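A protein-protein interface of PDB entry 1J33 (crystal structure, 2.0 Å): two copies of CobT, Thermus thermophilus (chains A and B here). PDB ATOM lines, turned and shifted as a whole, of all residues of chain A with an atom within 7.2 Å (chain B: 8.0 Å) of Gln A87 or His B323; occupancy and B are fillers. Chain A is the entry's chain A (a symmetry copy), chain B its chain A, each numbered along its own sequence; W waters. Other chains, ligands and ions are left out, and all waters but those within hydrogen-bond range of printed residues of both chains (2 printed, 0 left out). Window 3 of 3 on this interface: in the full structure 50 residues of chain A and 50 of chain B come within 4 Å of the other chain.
The guanidinium group (NE) of Arg B320 lies within hydrogen-bond range of the side-chain amide oxygen (OE1) of Gln A87, 2.7 Å away.
The backbone carbonyl oxygen (O) of Gly A82 lies within hydrogen-bond range of the backbone NH (N) of Ala B325 (2.9 Å).
Printed residues of chain B that touch a printed residue of chain A: Leu B23, Ala B317, Arg B320, Ile B321, His B323, Met B324 and Ala B325.
Of the 15 printed residues of chain A, 6 touch a printed residue of chain B.
Along chain A the printed residues that touch a printed residue of chain B span positions 82 to 90.
Among the printed residues, 11 pairs touch across the chains.
Among the printed residues, no Asp or Glu carboxylate lies within 4 Å of a Lys or Arg side-chain nitrogen of the other chain.
Of the printed residues of chain B, Gln A87 touches Arg B320, His B323 and Met B324.
Of chain A, only Gln A87 comes within 4 Å of His B323.
Of the printed residues of chain A, Ala B325 touches Gly A82 (2.9 Å).
Of the printed residues of chain A, Leu B23 touches Phe A88 (3.9 Å).
The nearest residue of chain B that does not touch Gln A87 is Ile B321 (4.9 Å).
The nearest printed residue of chain A that does not touch Ile B321 is Gln A87 (4.9 Å).
Water W1 lies within hydrogen-bond range of the guanidinium group (NH1) of Arg B316 and the backbone carbonyl oxygen (O) of Ala A91.
Water W2 bridges the side-chain amide nitrogen of Gln A87 and the guanidinium group of Arg B320.
NH2 of Arg B12 is in hydrogen-bond range of O of Met B324, 2.9 Å away.
O of Pro B42 is in hydrogen-bond range of NE2 of His B323, at 2.7 Å.
The backbone carbonyl oxygen (O) of Gly A81 sits at hydrogen-bond distance from the side-chain amide nitrogen (NE2) of Gln A87 (3.3 Å).
The backbone NH (N) of Ala A83 is in hydrogen-bond range of the side-chain amide oxygen (OD1) of Asn A86.
No position is printed for both chains.
Of the 11 pairs that touch across the chains among the printed residues, none has its exchanged pair printed and touching as well.
Met B324 touches Gly A82.
Met B324 touches Ala A83 (CG to C, 3.9 Å).
Met B324 touches Ala A84 (CE to N, 3.5 Å).
OE1 of Gln A87 touches CB of His B323, 3.5 Å away.
CG of Gln A87 touches CG of Met B324 (3.7 Å).
Phe A88 touches Leu B23.
Ala B317 touches Phe A88.
Ile B321 touches Phe A88 (CG1 to CE1, 3.7 Å).
CD2 of Leu A90 touches NH2 of Arg B320, 3.8 Å away.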
ATOM      1  N   ARG A  80     -39.169  -5.303  12.100  1.00  0.00           N
ATOM      2  CA  ARG A  80     -38.218  -5.999  11.248  1.00  0.00           C
ATOM      3  C   ARG A  80     -37.303  -6.930  12.037  1.00  0.00           C
ATOM      4  O   ARG A  80     -36.457  -7.603  11.459  1.00  0.00           O
ATOM      5  CB  ARG A  80     -37.417  -4.980  10.441  1.00  0.00           C
ATOM      6  CG  ARG A  80     -38.310  -4.238   9.456  1.00  0.00           C
ATOM      7  CD  ARG A  80     -37.700  -2.953   8.942  1.00  0.00           C
ATOM      8  NE  ARG A  80     -38.700  -2.153   8.239  1.00  0.00           N
ATOM      9  CZ  ARG A  80     -38.488  -0.926   7.776  1.00  0.00           C
ATOM     10  NH1 ARG A  80     -37.303  -0.351   7.942  1.00  0.00           N
ATOM     11  NH2 ARG A  80     -39.459  -0.274   7.151  1.00  0.00           N
ATOM     12  N   GLY A  81     -37.484  -6.959  13.356  1.00  0.00           N
ATOM     13  CA  GLY A  81     -36.705  -7.842  14.213  1.00  0.00           C
ATOM     14  C   GLY A  81     -35.271  -7.458  14.530  1.00  0.00           C
ATOM     15  O   GLY A  81     -34.494  -8.299  14.984  1.00  0.00           O
ATOM     16  N   GLY A  82     -34.916  -6.196  14.317  1.00  0.00           N
ATOM     17  CA  GLY A  82     -33.552  -5.770  14.584  1.00  0.00           C
ATOM     18  C   GLY A  82     -33.290  -5.133  15.938  1.00  0.00           C
ATOM     19  O   GLY A  82     -32.177  -4.643  16.191  1.00  0.00           O
ATOM     20  N   ALA A  83     -34.288  -5.139  16.818  1.00  0.00           N
ATOM     21  CA  ALA A  83     -34.125  -4.532  18.139  1.00  0.00           C
ATOM     22  C   ALA A  83     -33.783  -5.549  19.223  1.00  0.00           C
ATOM     23  O   ALA A  83     -33.915  -6.756  19.023  1.00  0.00           O
ATOM     24  CB  ALA A  83     -35.386  -3.768  18.521  1.00  0.00           C
ATOM     25  N   ALA A  84     -33.348  -5.054  20.378  1.00  0.00           N
ATOM     26  CA  ALA A  84     -32.984  -5.930  21.482  1.00  0.00           C
ATOM     27  C   ALA A  84     -34.166  -6.774  21.909  1.00  0.00           C
ATOM     28  O   ALA A  84     -34.032  -7.975  22.165  1.00  0.00           O
ATOM     29  CB  ALA A  84     -32.483  -5.115  22.662  1.00  0.00           C
ATOM     30  N   ILE A  85     -35.330  -6.144  21.991  1.00  0.00           N
ATOM     31  CA  ILE A  85     -36.517  -6.862  22.409  1.00  0.00           C
ATOM     32  C   ILE A  85     -36.782  -8.024  21.455  1.00  0.00           C
ATOM     33  O   ILE A  85     -37.246  -9.077  21.880  1.00  0.00           O
ATOM     34  CB  ILE A  85     -37.747  -5.920  22.485  1.00  0.00           C
ATOM     35  CG1 ILE A  85     -38.943  -6.677  23.068  1.00  0.00           C
ATOM     36  CG2 ILE A  85     -38.086  -5.373  21.102  1.00  0.00           C
ATOM     37  CD1 ILE A  85     -38.728  -7.165  24.489  1.00  0.00           C
ATOM     38  N   ASN A  86     -36.474  -7.853  20.170  1.00  0.00           N
ATOM     39  CA  ASN A  86     -36.690  -8.943  19.225  1.00  0.00           C
ATOM     40  C   ASN A  86     -35.747 -10.090  19.555  1.00  0.00           C
ATOM     41  O   ASN A  86     -36.148 -11.257  19.567  1.00  0.00           O
ATOM     42  CB  ASN A  86     -36.438  -8.500  17.779  1.00  0.00           C
ATOM     43  CG  ASN A  86     -37.355  -7.384  17.341  1.00  0.00           C
ATOM     44  OD1 ASN A  86     -36.964  -6.217  17.329  1.00  0.00           O
ATOM     45  ND2 ASN A  86     -38.589  -7.731  16.984  1.00  0.00           N
ATOM     46  N   GLN A  87     -34.490  -9.756  19.829  1.00  0.00           N
ATOM     47  CA  GLN A  87     -33.499 -10.775  20.140  1.00  0.00           C
ATOM     48  C   GLN A  87     -33.794 -11.529  21.428  1.00  0.00           C
ATOM     49  O   GLN A  87     -33.670 -12.756  21.474  1.00  0.00           O
ATOM     50  CB  GLN A  87     -32.100 -10.157  20.220  1.00  0.00           C
ATOM     51  CG  GLN A  87     -31.577  -9.581  18.909  1.00  0.00           C
ATOM     52  CD  GLN A  87     -31.735 -10.541  17.737  1.00  0.00           C
ATOM     53  OE1 GLN A  87     -31.344 -11.711  17.812  1.00  0.00           O
ATOM     54  NE2 GLN A  87     -32.311 -10.045  16.645  1.00  0.00           N
ATOM     55  N   PHE A  88     -34.184 -10.813  22.479  1.00  0.00           N
ATOM     56  CA  PHE A  88     -34.468 -11.482  23.745  1.00  0.00           C
ATOM     57  C   PHE A  88     -35.752 -12.302  23.682  1.00  0.00           C
ATOM     58  O   PHE A  88     -35.844 -13.364  24.299  1.00  0.00           O
ATOM     59  CB  PHE A  88     -34.550 -10.462  24.891  1.00  0.00           C
ATOM     60  CG  PHE A  88     -33.250  -9.746  25.167  1.00  0.00           C
ATOM     61  CD1 PHE A  88     -32.057 -10.175  24.582  1.00  0.00           C
ATOM     62  CD2 PHE A  88     -33.216  -8.644  26.024  1.00  0.00           C
ATOM     63  CE1 PHE A  88     -30.850  -9.520  24.843  1.00  0.00           C
ATOM     64  CE2 PHE A  88     -32.013  -7.982  26.291  1.00  0.00           C
ATOM     65  CZ  PHE A  88     -30.827  -8.422  25.699  1.00  0.00           C
ATOM     66  N   ALA A  89     -36.740 -11.821  22.930  1.00  0.00           N
ATOM     67  CA  ALA A  89     -38.006 -12.534  22.816  1.00  0.00           C
ATOM     68  C   ALA A  89     -37.800 -13.849  22.086  1.00  0.00           C
ATOM     69  O   ALA A  89     -38.495 -14.829  22.342  1.00  0.00           O
ATOM     70  CB  ALA A  89     -39.031 -11.679  22.078  1.00  0.00           C
ATOM     71  N   LEU A  90     -36.837 -13.865  21.176  1.00  0.00           N
ATOM     72  CA  LEU A  90     -36.528 -15.068  20.411  1.00  0.00           C
ATOM     73  C   LEU A  90     -35.918 -16.100  21.344  1.00  0.00           C
ATOM     74  O   LEU A  90     -36.180 -17.292  21.223  1.00  0.00           O
ATOM     75  CB  LEU A  90     -35.543 -14.740  19.285  1.00  0.00           C
ATOM     76  CG  LEU A  90     -34.942 -15.909  18.495  1.00  0.00           C
ATOM     77  CD1 LEU A  90     -36.050 -16.732  17.848  1.00  0.00           C
ATOM     78  CD2 LEU A  90     -33.986 -15.371  17.435  1.00  0.00           C
ATOM     79  N   ALA A  91     -35.107 -15.632  22.286  1.00  0.00           N
ATOM     80  CA  ALA A  91     -34.458 -16.525  23.233  1.00  0.00           C
ATOM     81  C   ALA A  91     -35.367 -16.929  24.394  1.00  0.00           C
ATOM     82  O   ALA A  91     -35.082 -17.897  25.097  1.00  0.00           O
ATOM     83  CB  ALA A  91     -33.194 -15.873  23.769  1.00  0.00           C
ATOM     84  N   ALA A  92     -36.465 -16.203  24.588  1.00  0.00           N
ATOM     85  CA  ALA A  92     -37.375 -16.502  25.690  1.00  0.00           C
ATOM     86  C   ALA A  92     -38.747 -17.056  25.289  1.00  0.00           C
ATOM     87  O   ALA A  92     -39.649 -17.116  26.123  1.00  0.00           O
ATOM     88  CB  ALA A  92     -37.556 -15.256  26.544  1.00  0.00           C
ATOM     89  N   VAL A  96     -43.964 -11.042  20.129  1.00  0.00           N
ATOM     90  CA  VAL A  96     -43.756  -9.602  20.181  1.00  0.00           C
ATOM     91  C   VAL A  96     -44.837  -8.843  19.421  1.00  0.00           C
ATOM     92  O   VAL A  96     -45.018  -9.042  18.222  1.00  0.00           O
ATOM     93  CB  VAL A  96     -42.398  -9.208  19.561  1.00  0.00           C
ATOM     94  CG1 VAL A  96     -42.210  -7.690  19.635  1.00  0.00           C
ATOM     95  CG2 VAL A  96     -41.263  -9.939  20.266  1.00  0.00           C
ATOM     96  N   VAL A 309     -38.746  -9.573  29.554  1.00  0.00           N
ATOM     97  CA  VAL A 309     -38.629 -10.749  28.714  1.00  0.00           C
ATOM     98  C   VAL A 309     -37.461 -11.616  29.159  1.00  0.00           C
ATOM     99  O   VAL A 309     -37.554 -12.840  29.136  1.00  0.00           O
ATOM    100  CB  VAL A 309     -38.457 -10.349  27.227  1.00  0.00           C
ATOM    101  CG1 VAL A 309     -38.303 -11.593  26.353  1.00  0.00           C
ATOM    102  CG2 VAL A 309     -39.674  -9.543  26.778  1.00  0.00           C
ATOM    103  N   ARG B  12     -18.897  -3.284  16.826  1.00  0.00           N
ATOM    104  CA  ARG B  12     -20.305  -3.476  16.487  1.00  0.00           C
ATOM    105  C   ARG B  12     -21.181  -3.177  17.703  1.00  0.00           C
ATOM    106  O   ARG B  12     -22.204  -2.503  17.591  1.00  0.00           O
ATOM    107  CB  ARG B  12     -20.564  -4.906  15.998  1.00  0.00           C
ATOM    108  CG  ARG B  12     -22.002  -5.123  15.530  1.00  0.00           C
ATOM    109  CD  ARG B  12     -22.259  -6.541  15.028  1.00  0.00           C
ATOM    110  NE  ARG B  12     -23.655  -6.745  14.635  1.00  0.00           N
ATOM    111  CZ  ARG B  12     -24.218  -6.220  13.548  1.00  0.00           C
ATOM    112  NH1 ARG B  12     -23.507  -5.459  12.728  1.00  0.00           N
ATOM    113  NH2 ARG B  12     -25.499  -6.452  13.280  1.00  0.00           N
ATOM    114  N   MET B  13     -20.768  -3.675  18.866  1.00  0.00           N
ATOM    115  CA  MET B  13     -21.507  -3.441  20.105  1.00  0.00           C
ATOM    116  C   MET B  13     -21.828  -1.952  20.260  1.00  0.00           C
ATOM    117  O   MET B  13     -22.950  -1.576  20.590  1.00  0.00           O
ATOM    118  CB  MET B  13     -20.675  -3.911  21.306  1.00  0.00           C
ATOM    119  CG  MET B  13     -21.328  -3.697  22.677  1.00  0.00           C
ATOM    120  SD  MET B  13     -22.884  -4.609  22.931  1.00  0.00           S
ATOM    121  CE  MET B  13     -22.264  -6.296  23.101  1.00  0.00           C
ATOM    122  N   LEU B  16     -24.807  -0.850  17.956  1.00  0.00           N
ATOM    123  CA  LEU B  16     -26.120  -1.484  18.038  1.00  0.00           C
ATOM    124  C   LEU B  16     -27.185  -0.434  18.352  1.00  0.00           C
ATOM    125  O   LEU B  16     -26.878   0.596  18.944  1.00  0.00           O
ATOM    126  CB  LEU B  16     -26.110  -2.582  19.108  1.00  0.00           C
ATOM    127  CG  LEU B  16     -25.122  -3.718  18.811  1.00  0.00           C
ATOM    128  CD1 LEU B  16     -25.275  -4.844  19.835  1.00  0.00           C
ATOM    129  CD2 LEU B  16     -25.380  -4.248  17.402  1.00  0.00           C
ATOM    130  N   LEU B  23     -27.354  -2.191  27.793  1.00  0.00           N
ATOM    131  CA  LEU B  23     -27.616  -3.582  28.163  1.00  0.00           C
ATOM    132  C   LEU B  23     -26.684  -4.078  29.274  1.00  0.00           C
ATOM    133  O   LEU B  23     -26.459  -5.278  29.447  1.00  0.00           O
ATOM    134  CB  LEU B  23     -27.556  -4.495  26.929  1.00  0.00           C
ATOM    135  CG  LEU B  23     -28.740  -4.278  25.968  1.00  0.00           C
ATOM    136  CD1 LEU B  23     -28.567  -5.138  24.731  1.00  0.00           C
ATOM    137  CD2 LEU B  23     -30.062  -4.618  26.660  1.00  0.00           C
ATOM    138  N   ALA B  30     -21.758 -10.835  26.241  1.00  0.00           N
ATOM    139  CA  ALA B  30     -21.855 -10.971  24.790  1.00  0.00           C
ATOM    140  C   ALA B  30     -20.468 -10.929  24.149  1.00  0.00           C
ATOM    141  O   ALA B  30     -20.152 -11.745  23.278  1.00  0.00           O
ATOM    142  CB  ALA B  30     -22.726  -9.855  24.218  1.00  0.00           C
ATOM    143  N   GLN B  37     -15.889 -17.852  20.749  1.00  0.00           N
ATOM    144  CA  GLN B  37     -16.212 -18.552  19.514  1.00  0.00           C
ATOM    145  C   GLN B  37     -15.495 -17.992  18.294  1.00  0.00           C
ATOM    146  O   GLN B  37     -15.562 -18.578  17.218  1.00  0.00           O
ATOM    147  CB  GLN B  37     -17.718 -18.509  19.263  1.00  0.00           C
ATOM    148  CG  GLN B  37     -18.568 -18.886  20.457  1.00  0.00           C
ATOM    149  CD  GLN B  37     -20.028 -19.055  20.084  1.00  0.00           C
ATOM    150  OE1 GLN B  37     -20.530 -18.376  19.193  1.00  0.00           O
ATOM    151  NE2 GLN B  37     -20.717 -19.955  20.774  1.00  0.00           N
ATOM    152  N   ARG B  39     -16.285 -15.353  16.787  1.00  0.00           N
ATOM    153  CA  ARG B  39     -17.368 -14.842  15.946  1.00  0.00           C
ATOM    154  C   ARG B  39     -17.805 -13.461  16.426  1.00  0.00           C
ATOM    155  O   ARG B  39     -17.728 -13.157  17.615  1.00  0.00           O
ATOM    156  CB  ARG B  39     -18.592 -15.756  16.029  1.00  0.00           C
ATOM    157  CG  ARG B  39     -18.539 -17.032  15.235  1.00  0.00           C
ATOM    158  CD  ARG B  39     -19.681 -17.944  15.666  1.00  0.00           C
ATOM    159  NE  ARG B  39     -19.847 -19.088  14.775  1.00  0.00           N
ATOM    160  CZ  ARG B  39     -20.602 -20.145  15.049  1.00  0.00           C
ATOM    161  NH1 ARG B  39     -21.261 -20.210  16.197  1.00  0.00           N
ATOM    162  NH2 ARG B  39     -20.710 -21.134  14.172  1.00  0.00           N
ATOM    163  N   VAL B  40     -18.276 -12.632  15.502  1.00  0.00           N
ATOM    164  CA  VAL B  40     -18.765 -11.308  15.857  1.00  0.00           C
ATOM    165  C   VAL B  40     -20.186 -11.511  16.380  1.00  0.00           C
ATOM    166  O   VAL B  40     -20.619 -10.849  17.324  1.00  0.00           O
ATOM    167  CB  VAL B  40     -18.788 -10.371  14.632  1.00  0.00           C
ATOM    168  CG1 VAL B  40     -19.467  -9.056  14.989  1.00  0.00           C
ATOM    169  CG2 VAL B  40     -17.364 -10.114  14.156  1.00  0.00           C
ATOM    170  N   LYS B  41     -20.904 -12.440  15.759  1.00  0.00           N
ATOM    171  CA  LYS B  41     -22.264 -12.758  16.169  1.00  0.00           C
ATOM    172  C   LYS B  41     -22.288 -14.177  16.737  1.00  0.00           C
ATOM    173  O   LYS B  41     -22.525 -15.142  16.014  1.00  0.00           O
ATOM    174  CB  LYS B  41     -23.218 -12.635  14.977  1.00  0.00           C
ATOM    175  CG  LYS B  41     -23.286 -11.228  14.409  1.00  0.00           C
ATOM    176  CD  LYS B  41     -24.349 -11.091  13.329  1.00  0.00           C
ATOM    177  CE  LYS B  41     -24.406  -9.658  12.814  1.00  0.00           C
ATOM    178  NZ  LYS B  41     -25.489  -9.444  11.814  1.00  0.00           N
ATOM    179  N   PRO B  42     -22.039 -14.315  18.050  1.00  0.00           N
ATOM    180  CA  PRO B  42     -22.013 -15.597  18.765  1.00  0.00           C
ATOM    181  C   PRO B  42     -23.274 -16.427  18.578  1.00  0.00           C
ATOM    182  O   PRO B  42     -24.373 -15.885  18.485  1.00  0.00           O
ATOM    183  CB  PRO B  42     -21.816 -15.179  20.222  1.00  0.00           C
ATOM    184  CG  PRO B  42     -21.046 -13.914  20.106  1.00  0.00           C
ATOM    185  CD  PRO B  42     -21.752 -13.204  18.975  1.00  0.00           C
ATOM    186  N   GLU B  43     -23.099 -17.744  18.533  1.00  0.00           N
ATOM    187  CA  GLU B  43     -24.200 -18.682  18.358  1.00  0.00           C
ATOM    188  C   GLU B  43     -24.281 -19.652  19.536  1.00  0.00           C
ATOM    189  O   GLU B  43     -23.275 -20.228  19.947  1.00  0.00           O
ATOM    190  CB  GLU B  43     -24.001 -19.501  17.081  1.00  0.00           C
ATOM    191  CG  GLU B  43     -24.022 -18.720  15.776  1.00  0.00           C
ATOM    192  CD  GLU B  43     -25.422 -18.377  15.317  1.00  0.00           C
ATOM    193  OE1 GLU B  43     -26.324 -19.233  15.458  1.00  0.00           O
ATOM    194  OE2 GLU B  43     -25.619 -17.260  14.796  1.00  0.00           O
ATOM    195  N   LEU B  44     -25.479 -19.837  20.075  1.00  0.00           N
ATOM    196  CA  LEU B  44     -25.669 -20.767  21.179  1.00  0.00           C
ATOM    197  C   LEU B  44     -26.981 -21.509  21.005  1.00  0.00           C
ATOM    198  O   LEU B  44     -27.945 -20.978  20.446  1.00  0.00           O
ATOM    199  CB  LEU B  44     -25.670 -20.043  22.529  1.00  0.00           C
ATOM    200  CG  LEU B  44     -24.335 -19.517  23.061  1.00  0.00           C
ATOM    201  CD1 LEU B  44     -24.551 -18.920  24.447  1.00  0.00           C
ATOM    202  CD2 LEU B  44     -23.314 -20.652  23.126  1.00  0.00           C
ATOM    203  N   ARG B 316     -27.796 -17.213  26.454  1.00  0.00           N
ATOM    204  CA  ARG B 316     -28.302 -17.274  25.088  1.00  0.00           C
ATOM    205  C   ARG B 316     -28.820 -15.895  24.692  1.00  0.00           C
ATOM    206  O   ARG B 316     -28.647 -15.455  23.558  1.00  0.00           O
ATOM    207  CB  ARG B 316     -29.434 -18.299  24.974  1.00  0.00           C
ATOM    208  CG  ARG B 316     -29.026 -19.718  25.309  1.00  0.00           C
ATOM    209  CD  ARG B 316     -30.039 -20.717  24.771  1.00  0.00           C
ATOM    210  NE  ARG B 316     -29.664 -22.092  25.088  1.00  0.00           N
ATOM    211  CZ  ARG B 316     -30.130 -22.774  26.128  1.00  0.00           C
ATOM    212  NH1 ARG B 316     -31.002 -22.211  26.956  1.00  0.00           N
ATOM    213  NH2 ARG B 316     -29.716 -24.017  26.348  1.00  0.00           N
ATOM    214  N   ALA B 317     -29.462 -15.207  25.630  1.00  0.00           N
ATOM    215  CA  ALA B 317     -29.974 -13.874  25.342  1.00  0.00           C
ATOM    216  C   ALA B 317     -28.800 -12.924  25.096  1.00  0.00           C
ATOM    217  O   ALA B 317     -28.857 -12.076  24.206  1.00  0.00           O
ATOM    218  CB  ALA B 317     -30.835 -13.375  26.501  1.00  0.00           C
ATOM    219  N   ALA B 318     -27.738 -13.060  25.889  1.00  0.00           N
ATOM    220  CA  ALA B 318     -26.565 -12.205  25.717  1.00  0.00           C
ATOM    221  C   ALA B 318     -25.931 -12.483  24.356  1.00  0.00           C
ATOM    222  O   ALA B 318     -25.490 -11.566  23.673  1.00  0.00           O
ATOM    223  CB  ALA B 318     -25.555 -12.466  26.823  1.00  0.00           C
ATOM    224  N   ALA B 319     -25.892 -13.756  23.967  1.00  0.00           N
ATOM    225  CA  ALA B 319     -25.316 -14.142  22.680  1.00  0.00           C
ATOM    226  C   ALA B 319     -26.044 -13.469  21.521  1.00  0.00           C
ATOM    227  O   ALA B 319     -25.447 -13.184  20.485  1.00  0.00           O
ATOM    228  CB  ALA B 319     -25.376 -15.654  22.516  1.00  0.00           C
ATOM    229  N   ARG B 320     -27.335 -13.214  21.697  1.00  0.00           N
ATOM    230  CA  ARG B 320     -28.127 -12.588  20.644  1.00  0.00           C
ATOM    231  C   ARG B 320     -27.949 -11.075  20.547  1.00  0.00           C
ATOM    232  O   ARG B 320     -28.332 -10.467  19.550  1.00  0.00           O
ATOM    233  CB  ARG B 320     -29.614 -12.903  20.839  1.00  0.00           C
ATOM    234  CG  ARG B 320     -29.969 -14.370  20.664  1.00  0.00           C
ATOM    235  CD  ARG B 320     -29.562 -14.892  19.292  1.00  0.00           C
ATOM    236  NE  ARG B 320     -30.203 -14.161  18.200  1.00  0.00           N
ATOM    237  CZ  ARG B 320     -30.195 -14.557  16.928  1.00  0.00           C
ATOM    238  NH1 ARG B 320     -29.576 -15.681  16.587  1.00  0.00           N
ATOM    239  NH2 ARG B 320     -30.809 -13.835  15.998  1.00  0.00           N
ATOM    240  N   ILE B 321     -27.372 -10.459  21.569  1.00  0.00           N
ATOM    241  CA  ILE B 321     -27.192  -9.010  21.539  1.00  0.00           C
ATOM    242  C   ILE B 321     -26.485  -8.498  20.280  1.00  0.00           C
ATOM    243  O   ILE B 321     -26.917  -7.521  19.670  1.00  0.00           O
ATOM    244  CB  ILE B 321     -26.432  -8.527  22.784  1.00  0.00           C
ATOM    245  CG1 ILE B 321     -27.336  -8.662  24.013  1.00  0.00           C
ATOM    246  CG2 ILE B 321     -25.982  -7.069  22.603  1.00  0.00           C
ATOM    247  CD1 ILE B 321     -26.658  -8.250  25.326  1.00  0.00           C
ATOM    248  N   LEU B 322     -25.406  -9.160  19.879  1.00  0.00           N
ATOM    249  CA  LEU B 322     -24.674  -8.720  18.701  1.00  0.00           C
ATOM    250  C   LEU B 322     -25.425  -9.000  17.392  1.00  0.00           C
ATOM    251  O   LEU B 322     -25.017  -8.540  16.330  1.00  0.00           O
ATOM    252  CB  LEU B 322     -23.273  -9.346  18.701  1.00  0.00           C
ATOM    253  CG  LEU B 322     -22.374  -8.648  19.737  1.00  0.00           C
ATOM    254  CD1 LEU B 322     -21.219  -9.529  20.164  1.00  0.00           C
ATOM    255  CD2 LEU B 322     -21.879  -7.334  19.161  1.00  0.00           C
ATOM    256  N   HIS B 323     -26.533  -9.731  17.479  1.00  0.00           N
ATOM    257  CA  HIS B 323     -27.356 -10.034  16.307  1.00  0.00           C
ATOM    258  C   HIS B 323     -28.332  -8.888  16.035  1.00  0.00           C
ATOM    259  O   HIS B 323     -29.032  -8.888  15.025  1.00  0.00           O
ATOM    260  CB  HIS B 323     -28.138 -11.330  16.521  1.00  0.00           C
ATOM    261  CG  HIS B 323     -27.279 -12.555  16.511  1.00  0.00           C
ATOM    262  ND1 HIS B 323     -27.048 -13.290  15.370  1.00  0.00           N
ATOM    263  CD2 HIS B 323     -26.572 -13.155  17.496  1.00  0.00           C
ATOM    264  CE1 HIS B 323     -26.235 -14.292  15.653  1.00  0.00           C
ATOM    265  NE2 HIS B 323     -25.931 -14.233  16.937  1.00  0.00           N
ATOM    266  N   MET B 324     -28.378  -7.923  16.954  1.00  0.00           N
ATOM    267  CA  MET B 324     -29.241  -6.748  16.814  1.00  0.00           C
ATOM    268  C   MET B 324     -28.724  -5.946  15.640  1.00  0.00           C
ATOM    269  O   MET B 324     -27.578  -6.105  15.238  1.00  0.00           O
ATOM    270  CB  MET B 324     -29.152  -5.849  18.049  1.00  0.00           C
ATOM    271  CG  MET B 324     -29.932  -6.299  19.272  1.00  0.00           C
ATOM    272  SD  MET B 324     -29.451  -5.262  20.685  1.00  0.00           S
ATOM    273  CE  MET B 324     -30.096  -3.666  20.168  1.00  0.00           C
ATOM    274  N   ALA B 325     -29.562  -5.062  15.114  1.00  0.00           N
ATOM    275  CA  ALA B 325     -29.163  -4.214  14.002  1.00  0.00           C
ATOM    276  C   ALA B 325     -28.381  -3.019  14.541  1.00  0.00           C
ATOM    277  O   ALA B 325     -28.574  -2.604  15.684  1.00  0.00           O
ATOM    278  CB  ALA B 325     -30.395  -3.725  13.254  1.00  0.00           C
ATOM    279  N   THR B 326     -27.482  -2.483  13.723  1.00  0.00           N
ATOM    280  CA  THR B 326     -26.722  -1.304  14.102  1.00  0.00           C
ATOM    281  C   THR B 326     -27.602  -0.151  13.641  1.00  0.00           C
ATOM    282  O   THR B 326     -28.610  -0.372  12.969  1.00  0.00           O
ATOM    283  CB  THR B 326     -25.374  -1.223  13.363  1.00  0.00           C
ATOM    284  OG1 THR B 326     -25.613  -1.193  11.952  1.00  0.00           O
ATOM    285  CG2 THR B 326     -24.506  -2.426  13.700  1.00  0.00           C
ATOM    286  N   GLU B 329     -27.718  -0.116   9.849  1.00  0.00           N
ATOM    287  CA  GLU B 329     -28.476  -1.260   9.354  1.00  0.00           C
ATOM    288  C   GLU B 329     -29.979  -1.092   9.563  1.00  0.00           C
ATOM    289  O   GLU B 329     -30.771  -1.623   8.790  1.00  0.00           O
ATOM    290  CB  GLU B 329     -28.012  -2.548  10.046  1.00  0.00           C
ATOM    291  CG  GLU B 329     -26.555  -2.943   9.759  1.00  0.00           C
ATOM    292  CD  GLU B 329     -26.107  -4.168  10.544  1.00  0.00           C
ATOM    293  OE1 GLU B 329     -24.935  -4.585  10.394  1.00  0.00           O
ATOM    294  OE2 GLU B 329     -26.919  -4.712  11.321  1.00  0.00           O
HETATM  295  O   HOH W   1     -32.933 -20.193  26.356  1.00  0.00           O
HETATM  296  O   HOH W   2     -32.801 -11.805  14.094  1.00  0.00           O
